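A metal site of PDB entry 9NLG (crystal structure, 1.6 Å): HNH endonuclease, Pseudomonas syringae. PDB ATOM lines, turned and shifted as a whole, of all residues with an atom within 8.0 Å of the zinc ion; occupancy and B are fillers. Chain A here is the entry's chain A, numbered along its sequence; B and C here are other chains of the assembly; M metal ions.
Four residues have an atom within 4 Å of the zinc ion: Cys 32, Cys 35, Cys 87 and Cys 90.
The zinc ion is bound by the side-chain sulfur (SG) of Cys 90, the side-chain sulfur (SG) of Cys 35, the side-chain sulfur (SG) of Cys 32 and the side-chain sulfur (SG) of Cys 87.
The backbone NH (N) of Thr 37 lies close to the side-chain sulfur (SG) of Cys 35 (3.7 Å). The side-chain sulfur (SG) of Cys 32 sits close to the backbone NH (N) of Leu 34, 3.4 Å away. The backbone NH (N) of Cys 32 is in hydrogen-bond range of the backbone carbonyl oxygen (O) of Thr 37 (2.9 Å).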
ATOM      1  N   HIS A  31      -1.445  22.924  21.472  1.00  0.00           N
ATOM      2  CA  HIS A  31      -2.793  23.085  20.967  1.00  0.00           C
ATOM      3  C   HIS A  31      -3.735  22.123  21.685  1.00  0.00           C
ATOM      4  O   HIS A  31      -3.331  21.055  22.129  1.00  0.00           O
ATOM      5  CB  HIS A  31      -2.873  22.825  19.468  1.00  0.00           C
ATOM      6  CG  HIS A  31      -2.314  23.920  18.630  1.00  0.00           C
ATOM      7  ND1 HIS A  31      -0.978  24.263  18.651  1.00  0.00           N
ATOM      8  CD2 HIS A  31      -2.905  24.746  17.719  1.00  0.00           C
ATOM      9  CE1 HIS A  31      -0.766  25.252  17.792  1.00  0.00           C
ATOM     10  NE2 HIS A  31      -1.919  25.556  17.214  1.00  0.00           N
ATOM     11  N   CYS A  32      -5.010  22.495  21.750  1.00  0.00           N
ATOM     12  CA  CYS A  32      -6.015  21.630  22.341  1.00  0.00           C
ATOM     13  C   CYS A  32      -6.226  20.396  21.477  1.00  0.00           C
ATOM     14  O   CYS A  32      -6.514  20.514  20.277  1.00  0.00           O
ATOM     15  CB  CYS A  32      -7.338  22.366  22.517  1.00  0.00           C
ATOM     16  SG  CYS A  32      -8.688  21.314  23.142  1.00  0.00           S
ATOM     17  N   GLU A  33      -6.104  19.221  22.095  1.00  0.00           N
ATOM     18  CA  GLU A  33      -6.183  17.991  21.327  1.00  0.00           C
ATOM     19  C   GLU A  33      -7.587  17.723  20.796  1.00  0.00           C
ATOM     20  O   GLU A  33      -7.730  16.940  19.848  1.00  0.00           O
ATOM     21  CB  GLU A  33      -5.724  16.811  22.194  1.00  0.00           C
ATOM     22  CG  GLU A  33      -4.262  16.912  22.606  1.00  0.00           C
ATOM     23  CD  GLU A  33      -3.773  15.646  23.260  1.00  0.00           C
ATOM     24  OE1 GLU A  33      -3.998  14.558  22.691  1.00  0.00           O
ATOM     25  OE2 GLU A  33      -3.155  15.761  24.343  1.00  0.00           O
ATOM     26  N   LEU A  34      -8.609  18.359  21.364  1.00  0.00           N
ATOM     27  CA  LEU A  34      -9.972  18.091  20.940  1.00  0.00           C
ATOM     28  C   LEU A  34     -10.567  19.152  20.009  1.00  0.00           C
ATOM     29  O   LEU A  34     -11.480  18.829  19.247  1.00  0.00           O
ATOM     30  CB  LEU A  34     -10.889  17.935  22.155  1.00  0.00           C
ATOM     31  CG  LEU A  34     -10.611  16.696  23.006  1.00  0.00           C
ATOM     32  CD1 LEU A  34     -11.496  16.653  24.256  1.00  0.00           C
ATOM     33  CD2 LEU A  34     -10.780  15.400  22.187  1.00  0.00           C
ATOM     34  N   CYS A  35     -10.070  20.392  20.045  1.00  0.00           N
ATOM     35  CA  CYS A  35     -10.577  21.396  19.123  1.00  0.00           C
ATOM     36  C   CYS A  35      -9.509  22.110  18.292  1.00  0.00           C
ATOM     37  O   CYS A  35      -9.873  22.846  17.375  1.00  0.00           O
ATOM     38  CB  CYS A  35     -11.425  22.445  19.863  1.00  0.00           C
ATOM     39  SG  CYS A  35     -10.478  23.608  20.869  1.00  0.00           S
ATOM     40  N   GLY A  36      -8.230  21.880  18.549  1.00  0.00           N
ATOM     41  CA  GLY A  36      -7.175  22.438  17.734  1.00  0.00           C
ATOM     42  C   GLY A  36      -6.799  23.887  18.018  1.00  0.00           C
ATOM     43  O   GLY A  36      -5.920  24.422  17.336  1.00  0.00           O
ATOM     44  N   THR A  37      -7.407  24.523  19.012  1.00  0.00           N
ATOM     45  CA  THR A  37      -7.100  25.926  19.267  1.00  0.00           C
ATOM     46  C   THR A  37      -5.700  26.064  19.868  1.00  0.00           C
ATOM     47  O   THR A  37      -5.204  25.162  20.554  1.00  0.00           O
ATOM     48  CB  THR A  37      -8.147  26.560  20.177  1.00  0.00           C
ATOM     49  OG1 THR A  37      -8.126  27.988  20.025  1.00  0.00           O
ATOM     50  CG2 THR A  37      -7.901  26.228  21.642  1.00  0.00           C
ATOM     51  N   ASP A  38      -5.055  27.196  19.569  1.00  0.00           N
ATOM     52  CA  ASP A  38      -3.706  27.498  20.041  1.00  0.00           C
ATOM     53  C   ASP A  38      -3.771  27.953  21.493  1.00  0.00           C
ATOM     54  O   ASP A  38      -4.393  28.979  21.798  1.00  0.00           O
ATOM     55  CB  ASP A  38      -3.100  28.573  19.143  1.00  0.00           C
ATOM     56  CG  ASP A  38      -1.687  28.970  19.532  1.00  0.00           C
ATOM     57  OD1 ASP A  38      -1.140  28.530  20.558  1.00  0.00           O
ATOM     58  OD2 ASP A  38      -1.103  29.772  18.763  1.00  0.00           O
ATOM     59  N   LEU A  39      -3.161  27.189  22.392  1.00  0.00           N
ATOM     60  CA  LEU A  39      -3.228  27.468  23.823  1.00  0.00           C
ATOM     61  C   LEU A  39      -2.013  28.233  24.333  1.00  0.00           C
ATOM     62  O   LEU A  39      -1.830  28.339  25.556  1.00  0.00           O
ATOM     63  CB  LEU A  39      -3.386  26.160  24.599  1.00  0.00           C
ATOM     64  CG  LEU A  39      -4.643  25.381  24.214  1.00  0.00           C
ATOM     65  CD1 LEU A  39      -4.625  23.972  24.784  1.00  0.00           C
ATOM     66  CD2 LEU A  39      -5.903  26.099  24.676  1.00  0.00           C
ATOM     67  N   TRP A  51      -2.756  29.097  28.356  1.00  0.00           N
ATOM     68  CA  TRP A  51      -4.097  29.015  28.904  1.00  0.00           C
ATOM     69  C   TRP A  51      -4.728  27.634  28.728  1.00  0.00           C
ATOM     70  O   TRP A  51      -5.917  27.475  29.006  1.00  0.00           O
ATOM     71  CB  TRP A  51      -4.982  30.131  28.319  1.00  0.00           C
ATOM     72  CG  TRP A  51      -5.230  30.132  26.837  1.00  0.00           C
ATOM     73  CD1 TRP A  51      -4.377  30.554  25.862  1.00  0.00           C
ATOM     74  CD2 TRP A  51      -6.441  29.758  26.179  1.00  0.00           C
ATOM     75  NE1 TRP A  51      -4.975  30.434  24.632  1.00  0.00           N
ATOM     76  CE2 TRP A  51      -6.242  29.947  24.802  1.00  0.00           C
ATOM     77  CE3 TRP A  51      -7.667  29.258  26.628  1.00  0.00           C
ATOM     78  CZ2 TRP A  51      -7.229  29.643  23.859  1.00  0.00           C
ATOM     79  CZ3 TRP A  51      -8.649  28.976  25.688  1.00  0.00           C
ATOM     80  CH2 TRP A  51      -8.421  29.167  24.318  1.00  0.00           C
ATOM     81  N   LEU A  85      -3.616  17.660  26.542  1.00  0.00           N
ATOM     82  CA  LEU A  85      -3.643  19.111  26.625  1.00  0.00           C
ATOM     83  C   LEU A  85      -4.988  19.580  26.062  1.00  0.00           C
ATOM     84  O   LEU A  85      -5.289  19.321  24.890  1.00  0.00           O
ATOM     85  CB  LEU A  85      -2.487  19.775  25.877  1.00  0.00           C
ATOM     86  CG  LEU A  85      -2.420  21.279  26.152  1.00  0.00           C
ATOM     87  CD1 LEU A  85      -2.021  21.582  27.605  1.00  0.00           C
ATOM     88  CD2 LEU A  85      -1.474  21.997  25.196  1.00  0.00           C
ATOM     89  N   LEU A  86      -5.772  20.266  26.883  1.00  0.00           N
ATOM     90  CA  LEU A  86      -7.096  20.707  26.475  1.00  0.00           C
ATOM     91  C   LEU A  86      -7.299  22.179  26.802  1.00  0.00           C
ATOM     92  O   LEU A  86      -6.701  22.716  27.747  1.00  0.00           O
ATOM     93  CB  LEU A  86      -8.199  19.927  27.176  1.00  0.00           C
ATOM     94  CG  LEU A  86      -8.180  18.412  27.010  1.00  0.00           C
ATOM     95  CD1 LEU A  86      -9.308  17.785  27.802  1.00  0.00           C
ATOM     96  CD2 LEU A  86      -8.297  18.077  25.544  1.00  0.00           C
ATOM     97  N   CYS A  87      -8.158  22.825  26.039  1.00  0.00           N
ATOM     98  CA  CYS A  87      -8.592  24.144  26.432  1.00  0.00           C
ATOM     99  C   CYS A  87      -9.548  24.021  27.606  1.00  0.00           C
ATOM    100  O   CYS A  87     -10.103  22.948  27.873  1.00  0.00           O
ATOM    101  CB  CYS A  87      -9.236  24.875  25.265  1.00  0.00           C
ATOM    102  SG  CYS A  87     -10.817  24.238  24.714  1.00  0.00           S
ATOM    103  N   PRO A  88      -9.732  25.104  28.354  1.00  0.00           N
ATOM    104  CA  PRO A  88     -10.605  25.018  29.534  1.00  0.00           C
ATOM    105  C   PRO A  88     -12.012  24.561  29.195  1.00  0.00           C
ATOM    106  O   PRO A  88     -12.614  23.774  29.949  1.00  0.00           O
ATOM    107  CB  PRO A  88     -10.584  26.451  30.079  1.00  0.00           C
ATOM    108  CG  PRO A  88      -9.281  27.033  29.583  1.00  0.00           C
ATOM    109  CD  PRO A  88      -9.060  26.408  28.234  1.00  0.00           C
ATOM    110  N   GLY A  89     -12.528  24.972  28.037  1.00  0.00           N
ATOM    111  CA  GLY A  89     -13.883  24.591  27.674  1.00  0.00           C
ATOM    112  C   GLY A  89     -14.014  23.115  27.371  1.00  0.00           C
ATOM    113  O   GLY A  89     -14.915  22.429  27.877  1.00  0.00           O
ATOM    114  N   CYS A  90     -13.114  22.580  26.540  1.00  0.00           N
ATOM    115  CA  CYS A  90     -13.185  21.146  26.237  1.00  0.00           C
ATOM    116  C   CYS A  90     -12.955  20.315  27.505  1.00  0.00           C
ATOM    117  O   CYS A  90     -13.611  19.288  27.701  1.00  0.00           O
ATOM    118  CB  CYS A  90     -12.190  20.758  25.152  1.00  0.00           C
ATOM    119  SG  CYS A  90     -12.515  21.461  23.476  1.00  0.00           S
ATOM    120  N   HIS A  91     -12.037  20.755  28.378  1.00  0.00           N
ATOM    121  CA  HIS A  91     -11.838  20.039  29.629  1.00  0.00           C
ATOM    122  C   HIS A  91     -13.118  20.032  30.468  1.00  0.00           C
ATOM    123  O   HIS A  91     -13.486  19.005  31.056  1.00  0.00           O
ATOM    124  CB  HIS A  91     -10.705  20.658  30.443  1.00  0.00           C
ATOM    125  CG  HIS A  91     -10.186  19.775  31.539  1.00  0.00           C
ATOM    126  ND1 HIS A  91      -9.198  20.171  32.416  1.00  0.00           N
ATOM    127  CD2 HIS A  91     -10.526  18.510  31.907  1.00  0.00           C
ATOM    128  CE1 HIS A  91      -8.952  19.189  33.265  1.00  0.00           C
ATOM    129  NE2 HIS A  91      -9.736  18.168  32.978  1.00  0.00           N
ATOM    130  N   LYS A  93     -16.223  20.265  29.499  1.00  0.00           N
ATOM    131  CA  LYS A  93     -17.219  19.396  28.899  1.00  0.00           C
ATOM    132  C   LYS A  93     -16.922  17.915  29.132  1.00  0.00           C
ATOM    133  O   LYS A  93     -17.834  17.148  29.450  1.00  0.00           O
ATOM    134  CB  LYS A  93     -17.323  19.718  27.413  1.00  0.00           C
ATOM    135  CG  LYS A  93     -17.979  21.054  27.132  1.00  0.00           C
ATOM    136  CD  LYS A  93     -17.671  21.529  25.719  1.00  0.00           C
ATOM    137  CE  LYS A  93     -18.278  22.865  25.431  1.00  0.00           C
ATOM    138  NZ  LYS A  93     -17.837  23.370  24.087  1.00  0.00           N
ATOM    139  N   ARG B  44     -21.153  19.060  21.009  1.00  0.00           N
ATOM    140  CA  ARG B  44     -20.338  17.985  20.463  1.00  0.00           C
ATOM    141  C   ARG B  44     -20.878  16.610  20.839  1.00  0.00           C
ATOM    142  O   ARG B  44     -20.960  15.721  19.988  1.00  0.00           O
ATOM    143  CB  ARG B  44     -18.889  18.118  20.924  1.00  0.00           C
ATOM    144  CG  ARG B  44     -18.032  16.923  20.536  1.00  0.00           C
ATOM    145  CD  ARG B  44     -16.539  17.150  20.802  1.00  0.00           C
ATOM    146  NE  ARG B  44     -15.779  15.969  20.399  1.00  0.00           N
ATOM    147  CZ  ARG B  44     -14.515  15.986  19.994  1.00  0.00           C
ATOM    148  NH1 ARG B  44     -13.811  17.103  20.001  1.00  0.00           N
ATOM    149  NH2 ARG B  44     -13.965  14.860  19.567  1.00  0.00           N
ATOM    150  N   PRO C 124      -7.747  18.931  14.534  1.00  0.00           N
ATOM    151  CA  PRO C 124      -9.069  18.704  15.136  1.00  0.00           C
ATOM    152  C   PRO C 124     -10.132  19.673  14.652  1.00  0.00           C
ATOM    153  O   PRO C 124     -11.314  19.297  14.625  1.00  0.00           O
ATOM    154  CB  PRO C 124      -8.813  18.822  16.638  1.00  0.00           C
ATOM    155  CG  PRO C 124      -7.390  18.383  16.787  1.00  0.00           C
ATOM    156  CD  PRO C 124      -6.693  18.958  15.563  1.00  0.00           C
HETATM  157 ZN    ZN M   1     -10.586  22.658  22.992  1.00  0.00          ZN
